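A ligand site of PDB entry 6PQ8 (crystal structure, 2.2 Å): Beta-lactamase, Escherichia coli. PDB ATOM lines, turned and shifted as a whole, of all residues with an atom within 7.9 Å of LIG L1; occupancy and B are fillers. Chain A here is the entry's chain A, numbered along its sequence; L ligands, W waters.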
ATOM      1  N   THR A  25     -16.091 -13.547  25.934  1.00  0.00           N
ATOM      2  CA  THR A  25     -17.170 -12.812  25.284  1.00  0.00           C
ATOM      3  C   THR A  25     -16.700 -12.116  24.016  1.00  0.00           C
ATOM      4  O   THR A  25     -17.396 -12.136  22.996  1.00  0.00           O
ATOM      5  CB  THR A  25     -17.784 -11.803  26.262  1.00  0.00           C
ATOM      6  OG1 THR A  25     -18.189 -12.479  27.464  1.00  0.00           O
ATOM      7  CG2 THR A  25     -19.005 -11.111  25.639  1.00  0.00           C
ATOM      8  N   VAL A  47     -27.656 -10.059  23.906  1.00  0.00           N
ATOM      9  CA  VAL A  47     -27.836 -11.192  24.809  1.00  0.00           C
ATOM     10  C   VAL A  47     -27.710 -10.700  26.242  1.00  0.00           C
ATOM     11  O   VAL A  47     -26.824  -9.909  26.555  1.00  0.00           O
ATOM     12  CB  VAL A  47     -26.795 -12.309  24.557  1.00  0.00           C
ATOM     13  CG1 VAL A  47     -27.005 -13.448  25.548  1.00  0.00           C
ATOM     14  CG2 VAL A  47     -26.830 -12.816  23.102  1.00  0.00           C
ATOM     15  N   LEU A  48     -28.591 -11.188  27.104  1.00  0.00           N
ATOM     16  CA  LEU A  48     -28.522 -10.879  28.537  1.00  0.00           C
ATOM     17  C   LEU A  48     -28.761 -12.150  29.336  1.00  0.00           C
ATOM     18  O   LEU A  48     -29.822 -12.783  29.187  1.00  0.00           O
ATOM     19  CB  LEU A  48     -29.549  -9.824  28.908  1.00  0.00           C
ATOM     20  CG  LEU A  48     -29.233  -8.849  30.018  1.00  0.00           C
ATOM     21  CD1 LEU A  48     -27.754  -8.493  30.001  1.00  0.00           C
ATOM     22  CD2 LEU A  48     -30.117  -7.613  29.879  1.00  0.00           C
ATOM     23  N   GLY A  49     -27.805 -12.543  30.167  1.00  0.00           N
ATOM     24  CA  GLY A  49     -28.036 -13.634  31.096  1.00  0.00           C
ATOM     25  C   GLY A  49     -29.156 -13.308  32.067  1.00  0.00           C
ATOM     26  O   GLY A  49     -29.331 -12.154  32.462  1.00  0.00           O
ATOM     27  N   ILE A  50     -29.931 -14.295  32.430  1.00  0.00           N
ATOM     28  CA  ILE A  50     -31.009 -14.069  33.343  1.00  0.00           C
ATOM     29  C   ILE A  50     -30.567 -14.133  34.779  1.00  0.00           C
ATOM     30  O   ILE A  50     -30.781 -13.212  35.510  1.00  0.00           O
ATOM     31  CB  ILE A  50     -32.156 -15.043  33.093  1.00  0.00           C
ATOM     32  CG1 ILE A  50     -32.771 -14.752  31.754  1.00  0.00           C
ATOM     33  CG2 ILE A  50     -33.216 -14.927  34.163  1.00  0.00           C
ATOM     34  CD1 ILE A  50     -33.345 -13.378  31.668  1.00  0.00           C
ATOM     35  N   GLU A  51     -29.956 -15.216  35.175  1.00  0.00           N
ATOM     36  CA  GLU A  51     -29.536 -15.352  36.541  1.00  0.00           C
ATOM     37  C   GLU A  51     -28.060 -15.111  36.801  1.00  0.00           C
ATOM     38  O   GLU A  51     -27.674 -14.822  37.885  1.00  0.00           O
ATOM     39  CB  GLU A  51     -30.131 -16.586  37.216  1.00  0.00           C
ATOM     40  CG  GLU A  51     -30.136 -17.897  36.481  1.00  0.00           C
ATOM     41  CD  GLU A  51     -31.107 -17.993  35.327  1.00  0.00           C
ATOM     42  OE1 GLU A  51     -32.315 -18.109  35.504  1.00  0.00           O
ATOM     43  OE2 GLU A  51     -30.627 -18.036  34.226  1.00  0.00           O
ATOM     44  N   ASP A  52     -27.252 -15.193  35.769  1.00  0.00           N
ATOM     45  CA  ASP A  52     -25.834 -14.983  35.870  1.00  0.00           C
ATOM     46  C   ASP A  52     -25.549 -13.936  34.873  1.00  0.00           C
ATOM     47  O   ASP A  52     -25.559 -14.196  33.713  1.00  0.00           O
ATOM     48  CB  ASP A  52     -25.065 -16.233  35.444  1.00  0.00           C
ATOM     49  CG  ASP A  52     -24.977 -17.283  36.551  1.00  0.00           C
ATOM     50  OD1 ASP A  52     -25.588 -17.128  37.601  1.00  0.00           O
ATOM     51  OD2 ASP A  52     -24.280 -18.266  36.358  1.00  0.00           O
ATOM     52  N   ASN A  53     -25.274 -12.743  35.338  1.00  0.00           N
ATOM     53  CA  ASN A  53     -25.024 -11.651  34.432  1.00  0.00           C
ATOM     54  C   ASN A  53     -23.977 -11.867  33.324  1.00  0.00           C
ATOM     55  O   ASN A  53     -22.803 -12.018  33.545  1.00  0.00           O
ATOM     56  CB  ASN A  53     -24.762 -10.387  35.203  1.00  0.00           C
ATOM     57  CG  ASN A  53     -23.316 -10.189  35.450  1.00  0.00           C
ATOM     58  OD1 ASN A  53     -22.670 -10.990  36.120  1.00  0.00           O
ATOM     59  ND2 ASN A  53     -22.788  -9.137  34.874  1.00  0.00           N
ATOM     60  N   PHE A  54     -24.477 -11.905  32.120  1.00  0.00           N
ATOM     61  CA  PHE A  54     -23.726 -12.089  30.930  1.00  0.00           C
ATOM     62  C   PHE A  54     -24.279 -11.082  29.946  1.00  0.00           C
ATOM     63  O   PHE A  54     -25.466 -10.865  29.876  1.00  0.00           O
ATOM     64  CB  PHE A  54     -23.905 -13.488  30.417  1.00  0.00           C
ATOM     65  CG  PHE A  54     -23.373 -13.692  29.071  1.00  0.00           C
ATOM     66  CD1 PHE A  54     -22.064 -13.999  28.889  1.00  0.00           C
ATOM     67  CD2 PHE A  54     -24.167 -13.552  27.985  1.00  0.00           C
ATOM     68  CE1 PHE A  54     -21.554 -14.180  27.638  1.00  0.00           C
ATOM     69  CE2 PHE A  54     -23.669 -13.711  26.730  1.00  0.00           C
ATOM     70  CZ  PHE A  54     -22.354 -14.032  26.556  1.00  0.00           C
ATOM     71  N   LYS A  55     -23.415 -10.472  29.184  1.00  0.00           N
ATOM     72  CA  LYS A  55     -23.853  -9.448  28.274  1.00  0.00           C
ATOM     73  C   LYS A  55     -23.154  -9.481  26.929  1.00  0.00           C
ATOM     74  O   LYS A  55     -21.953  -9.560  26.880  1.00  0.00           O
ATOM     75  CB  LYS A  55     -23.667  -8.123  28.964  1.00  0.00           C
ATOM     76  CG  LYS A  55     -24.052  -6.920  28.173  1.00  0.00           C
ATOM     77  CD  LYS A  55     -24.226  -5.726  29.083  1.00  0.00           C
ATOM     78  CE  LYS A  55     -23.793  -4.459  28.397  1.00  0.00           C
ATOM     79  NZ  LYS A  55     -22.536  -3.922  28.957  1.00  0.00           N
ATOM     80  N   ILE A 257     -34.342 -18.230  26.314  1.00  0.00           N
ATOM     81  CA  ILE A 257     -33.958 -19.600  26.012  1.00  0.00           C
ATOM     82  C   ILE A 257     -33.490 -20.297  27.277  1.00  0.00           C
ATOM     83  O   ILE A 257     -32.821 -19.686  28.121  1.00  0.00           O
ATOM     84  CB  ILE A 257     -32.852 -19.603  24.928  1.00  0.00           C
ATOM     85  CG1 ILE A 257     -33.376 -18.863  23.683  1.00  0.00           C
ATOM     86  CG2 ILE A 257     -32.357 -21.028  24.628  1.00  0.00           C
ATOM     87  CD1 ILE A 257     -32.705 -19.270  22.409  1.00  0.00           C
ATOM     88  N   LEU A 259     -31.137 -23.002  28.968  1.00  0.00           N
ATOM     89  CA  LEU A 259     -29.889 -23.719  28.808  1.00  0.00           C
ATOM     90  C   LEU A 259     -30.002 -25.114  29.417  1.00  0.00           C
ATOM     91  O   LEU A 259     -30.881 -25.370  30.245  1.00  0.00           O
ATOM     92  CB  LEU A 259     -28.753 -22.947  29.473  1.00  0.00           C
ATOM     93  CG  LEU A 259     -28.309 -21.659  28.790  1.00  0.00           C
ATOM     94  CD1 LEU A 259     -27.877 -20.621  29.829  1.00  0.00           C
ATOM     95  CD2 LEU A 259     -27.184 -21.971  27.803  1.00  0.00           C
ATOM     96  N   PRO A 260     -29.122 -26.044  29.021  1.00  0.00           N
ATOM     97  CA  PRO A 260     -29.200 -27.411  29.561  1.00  0.00           C
ATOM     98  C   PRO A 260     -29.147 -27.483  31.070  1.00  0.00           C
ATOM     99  O   PRO A 260     -29.761 -28.386  31.661  1.00  0.00           O
ATOM    100  CB  PRO A 260     -27.991 -28.104  28.916  1.00  0.00           C
ATOM    101  CG  PRO A 260     -27.807 -27.375  27.622  1.00  0.00           C
ATOM    102  CD  PRO A 260     -28.110 -25.941  27.946  1.00  0.00           C
ATOM    103  N   ASN A 261     -28.434 -26.573  31.728  1.00  0.00           N
ATOM    104  CA  ASN A 261     -28.362 -26.568  33.180  1.00  0.00           C
ATOM    105  C   ASN A 261     -29.570 -25.917  33.826  1.00  0.00           C
ATOM    106  O   ASN A 261     -29.550 -25.685  35.044  1.00  0.00           O
ATOM    107  CB  ASN A 261     -27.077 -25.884  33.648  1.00  0.00           C
ATOM    108  CG  ASN A 261     -27.052 -24.398  33.355  1.00  0.00           C
ATOM    109  OD1 ASN A 261     -27.956 -23.853  32.709  1.00  0.00           O
ATOM    110  ND2 ASN A 261     -26.015 -23.730  33.832  1.00  0.00           N
ATOM    111  N   GLY A 262     -30.609 -25.573  33.064  1.00  0.00           N
ATOM    112  CA  GLY A 262     -31.781 -24.966  33.643  1.00  0.00           C
ATOM    113  C   GLY A 262     -31.719 -23.463  33.809  1.00  0.00           C
ATOM    114  O   GLY A 262     -32.743 -22.859  34.189  1.00  0.00           O
ATOM    115  N   LYS A 263     -30.582 -22.832  33.547  1.00  0.00           N
ATOM    116  CA  LYS A 263     -30.522 -21.382  33.522  1.00  0.00           C
ATOM    117  C   LYS A 263     -31.074 -20.850  32.189  1.00  0.00           C
ATOM    118  O   LYS A 263     -31.400 -21.615  31.276  1.00  0.00           O
ATOM    119  CB  LYS A 263     -29.085 -20.922  33.743  1.00  0.00           C
ATOM    120  CG  LYS A 263     -28.665 -21.028  35.199  1.00  0.00           C
ATOM    121  CD  LYS A 263     -27.206 -20.690  35.392  1.00  0.00           C
ATOM    122  CE  LYS A 263     -26.786 -20.888  36.837  1.00  0.00           C
ATOM    123  NZ  LYS A 263     -25.301 -20.925  36.968  1.00  0.00           N
ATOM    124  N   HIS A 264     -31.169 -19.523  32.075  1.00  0.00           N
ATOM    125  CA  HIS A 264     -31.791 -18.874  30.925  1.00  0.00           C
ATOM    126  C   HIS A 264     -30.972 -17.677  30.456  1.00  0.00           C
ATOM    127  O   HIS A 264     -30.181 -17.103  31.215  1.00  0.00           O
ATOM    128  CB  HIS A 264     -33.217 -18.409  31.251  1.00  0.00           C
ATOM    129  CG  HIS A 264     -34.087 -19.484  31.823  1.00  0.00           C
ATOM    130  ND1 HIS A 264     -34.044 -19.835  33.154  1.00  0.00           N
ATOM    131  CD2 HIS A 264     -35.009 -20.295  31.242  1.00  0.00           C
ATOM    132  CE1 HIS A 264     -34.910 -20.819  33.372  1.00  0.00           C
ATOM    133  NE2 HIS A 264     -35.497 -21.117  32.232  1.00  0.00           N
ATOM    134  N   PHE A 265     -31.190 -17.290  29.189  1.00  0.00           N
ATOM    135  CA  PHE A 265     -30.672 -16.040  28.641  1.00  0.00           C
ATOM    136  C   PHE A 265     -31.718 -15.402  27.709  1.00  0.00           C
ATOM    137  O   PHE A 265     -32.463 -16.095  27.019  1.00  0.00           O
ATOM    138  CB  PHE A 265     -29.321 -16.224  27.917  1.00  0.00           C
ATOM    139  CG  PHE A 265     -29.354 -17.164  26.717  1.00  0.00           C
ATOM    140  CD1 PHE A 265     -29.209 -18.532  26.869  1.00  0.00           C
ATOM    141  CD2 PHE A 265     -29.458 -16.656  25.419  1.00  0.00           C
ATOM    142  CE1 PHE A 265     -29.195 -19.398  25.771  1.00  0.00           C
ATOM    143  CE2 PHE A 265     -29.455 -17.502  24.317  1.00  0.00           C
ATOM    144  CZ  PHE A 265     -29.327 -18.869  24.495  1.00  0.00           C
ATOM    145  N   ALA A 266     -31.780 -14.080  27.736  1.00  0.00           N
ATOM    146  CA  ALA A 266     -32.574 -13.307  26.787  1.00  0.00           C
ATOM    147  C   ALA A 266     -31.704 -12.932  25.588  1.00  0.00           C
ATOM    148  O   ALA A 266     -30.543 -12.575  25.741  1.00  0.00           O
ATOM    149  CB  ALA A 266     -33.147 -12.058  27.440  1.00  0.00           C
ATOM    150  N   VAL A 292     -24.104 -18.435  20.307  1.00  0.00           N
ATOM    151  CA  VAL A 292     -24.265 -17.966  21.691  1.00  0.00           C
ATOM    152  C   VAL A 292     -24.589 -19.136  22.608  1.00  0.00           C
ATOM    153  O   VAL A 292     -24.026 -19.263  23.702  1.00  0.00           O
ATOM    154  CB  VAL A 292     -25.347 -16.875  21.770  1.00  0.00           C
ATOM    155  CG1 VAL A 292     -25.624 -16.512  23.226  1.00  0.00           C
ATOM    156  CG2 VAL A 292     -24.922 -15.646  20.975  1.00  0.00           C
ATOM    157  N   TYR A 295     -21.399 -21.165  23.326  1.00  0.00           N
ATOM    158  CA  TYR A 295     -20.531 -20.480  24.277  1.00  0.00           C
ATOM    159  C   TYR A 295     -21.009 -20.670  25.719  1.00  0.00           C
ATOM    160  O   TYR A 295     -20.223 -21.027  26.598  1.00  0.00           O
ATOM    161  CB  TYR A 295     -20.458 -18.995  23.931  1.00  0.00           C
ATOM    162  CG  TYR A 295     -19.602 -18.212  24.889  1.00  0.00           C
ATOM    163  CD1 TYR A 295     -18.222 -18.206  24.769  1.00  0.00           C
ATOM    164  CD2 TYR A 295     -20.177 -17.471  25.919  1.00  0.00           C
ATOM    165  CE1 TYR A 295     -17.423 -17.488  25.647  1.00  0.00           C
ATOM    166  CE2 TYR A 295     -19.389 -16.752  26.806  1.00  0.00           C
ATOM    167  CZ  TYR A 295     -18.016 -16.768  26.666  1.00  0.00           C
ATOM    168  OH  TYR A 295     -17.235 -16.050  27.545  1.00  0.00           O
ATOM    169  N   LEU A 296     -22.300 -20.411  25.979  1.00  0.00           N
ATOM    170  CA  LEU A 296     -22.794 -20.475  27.353  1.00  0.00           C
ATOM    171  C   LEU A 296     -22.886 -21.914  27.855  1.00  0.00           C
ATOM    172  O   LEU A 296     -22.777 -22.155  29.065  1.00  0.00           O
ATOM    173  CB  LEU A 296     -24.163 -19.795  27.445  1.00  0.00           C
ATOM    174  CG  LEU A 296     -24.239 -18.327  27.027  1.00  0.00           C
ATOM    175  CD1 LEU A 296     -25.687 -17.857  26.970  1.00  0.00           C
ATOM    176  CD2 LEU A 296     -23.416 -17.445  27.945  1.00  0.00           C
ATOM    177  N   VAL A 297     -23.077 -22.876  26.953  1.00  0.00           N
ATOM    178  CA  VAL A 297     -23.066 -24.275  27.357  1.00  0.00           C
ATOM    179  C   VAL A 297     -21.658 -24.702  27.756  1.00  0.00           C
ATOM    180  O   VAL A 297     -21.466 -25.436  28.730  1.00  0.00           O
ATOM    181  CB  VAL A 297     -23.622 -25.146  26.208  1.00  0.00           C
ATOM    182  CG1 VAL A 297     -23.259 -26.589  26.416  1.00  0.00           C
ATOM    183  CG2 VAL A 297     -25.123 -24.981  26.099  1.00  0.00           C
ATOM    184  N   LYS A 298     -20.653 -24.246  27.013  1.00  0.00           N
ATOM    185  CA  LYS A 298     -19.248 -24.542  27.307  1.00  0.00           C
ATOM    186  C   LYS A 298     -18.770 -23.713  28.495  1.00  0.00           C
ATOM    187  O   LYS A 298     -18.348 -24.224  29.533  1.00  0.00           O
ATOM    188  CB  LYS A 298     -18.386 -24.274  26.066  1.00  0.00           C
ATOM    189  CG  LYS A 298     -16.895 -24.465  26.274  1.00  0.00           C
ATOM    190  CD  LYS A 298     -16.159 -24.660  24.942  1.00  0.00           C
ATOM    191  CE  LYS A 298     -15.685 -26.104  24.762  1.00  0.00           C
ATOM    192  NZ  LYS A 298     -14.835 -26.611  25.877  1.00  0.00           N
HETATM  193  O1  LIG L   1     -27.602 -17.618  33.073  1.00  0.00           O
HETATM  194  C1  LIG L   1     -26.613 -17.528  32.405  1.00  0.00           C
HETATM  195  C2  LIG L   1     -25.940 -16.439  31.580  1.00  0.00           C
HETATM  196  C3  LIG L   1     -25.008 -17.568  31.095  1.00  0.00           C
HETATM  197  N1  LIG L   1     -25.586 -18.454  32.122  1.00  0.00           N
HETATM  198  O2  LIG L   1     -23.614 -17.347  31.423  1.00  0.00           O
HETATM  199  C4  LIG L   1     -23.286 -18.410  32.166  1.00  0.00           C
HETATM  200  C5  LIG L   1     -24.478 -18.867  32.971  1.00  0.00           C
HETATM  201  C6  LIG L   1     -24.336 -20.382  33.156  1.00  0.00           C
HETATM  202  O3  LIG L   1     -24.933 -21.131  32.424  1.00  0.00           O
HETATM  203  O4  LIG L   1     -23.586 -20.783  34.013  1.00  0.00           O
HETATM  204  C7  LIG L   1     -21.996 -18.955  32.121  1.00  0.00           C
HETATM  205  C8  LIG L   1     -21.092 -18.529  30.997  1.00  0.00           C
HETATM  206  O5  LIG L   1     -21.044 -17.108  30.957  1.00  0.00           O
HETATM  207  N1  LG2 L   2     -20.354 -21.675  30.236  1.00  0.00           N
HETATM  208  C1  LG2 L   2     -19.453 -21.934  31.354  1.00  0.00           C
HETATM  209  C2  LG2 L   2     -20.069 -21.547  32.686  1.00  0.00           C
HETATM  210  O1  LG2 L   2     -21.242 -21.825  32.941  1.00  0.00           O
HETATM  211  C3  LG2 L   2     -18.128 -21.194  31.155  1.00  0.00           C
HETATM  212  C4  LG2 L   2     -17.001 -21.828  31.931  1.00  0.00           C
HETATM  213  O2  LG2 L   2     -17.230 -22.883  32.548  1.00  0.00           O
HETATM  214  O3  LG2 L   2     -15.882 -21.269  31.906  1.00  0.00           O
HETATM  215  O   HOH W   1     -24.456 -23.026  30.744  1.00  0.00           O
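An oxygen (O4) of LIG L1 lies within salt-bridge range of the side-chain amino group of Lys 263.
O of Lys 298 lies close to N1 of LG2 L2 (3.3 Å).
The side-chain amide nitrogen of Asn 261 is in hydrogen-bond range of an oxygen (O3) of LIG L1.
O of Leu 296 sits at hydrogen-bond distance from N1 of LG2 L2, at 2.7 Å.
An oxygen (O1) of LG2 L2 lies close to an oxygen (O4) of LIG L1 (2.8 Å).
N of His 264 lies within hydrogen-bond range of OE2 of Glu 51.
The side-chain amide oxygen (OD1) of Asn 261 lies within hydrogen-bond range of the backbone NH (N) of Lys 263 (2.9 Å).
The backbone NH (N) of Ile 50 sits at hydrogen-bond distance from the backbone carbonyl oxygen (O) of His 264 (3.1 Å).
ND1 of His 264 lies close to O of Gly 262, at 3.5 Å.
The backbone NH of Gly 49 sits at hydrogen-bond distance from the backbone carbonyl oxygen of Phe 54 (2.9 Å).
The side-chain carboxylate (OD2) of Asp 52 lies within salt-bridge range of the side-chain amino group (NZ) of Lys 263 (2.9 Å).
O1 of LIG L1 sits close to OE2 of Glu 51 (3.3 Å).
O1 of LIG L1 sits close to O of His 264, 3.2 Å away.
Gly 49 touches LIG L1.
Asp 52 touches LIG L1.
Phe 54 touches LIG L1 (CB to C2, 3.8 Å).
Leu 259 touches LIG L1 (CD1 to N1, 3.9 Å).
CD2 of Leu 296 touches O2 of LIG L1, at 3.5 Å.
Nine residues have an atom within 4 Å of LIG L1: Gly 49, Glu 51, Asp 52, Phe 54, Leu 259, Asn 261, Lys 263, His 264 and Leu 296.
Water W1 bridges O of Leu 296 (2.5 Å) and O3 of LIG L1 (2.6 Å).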
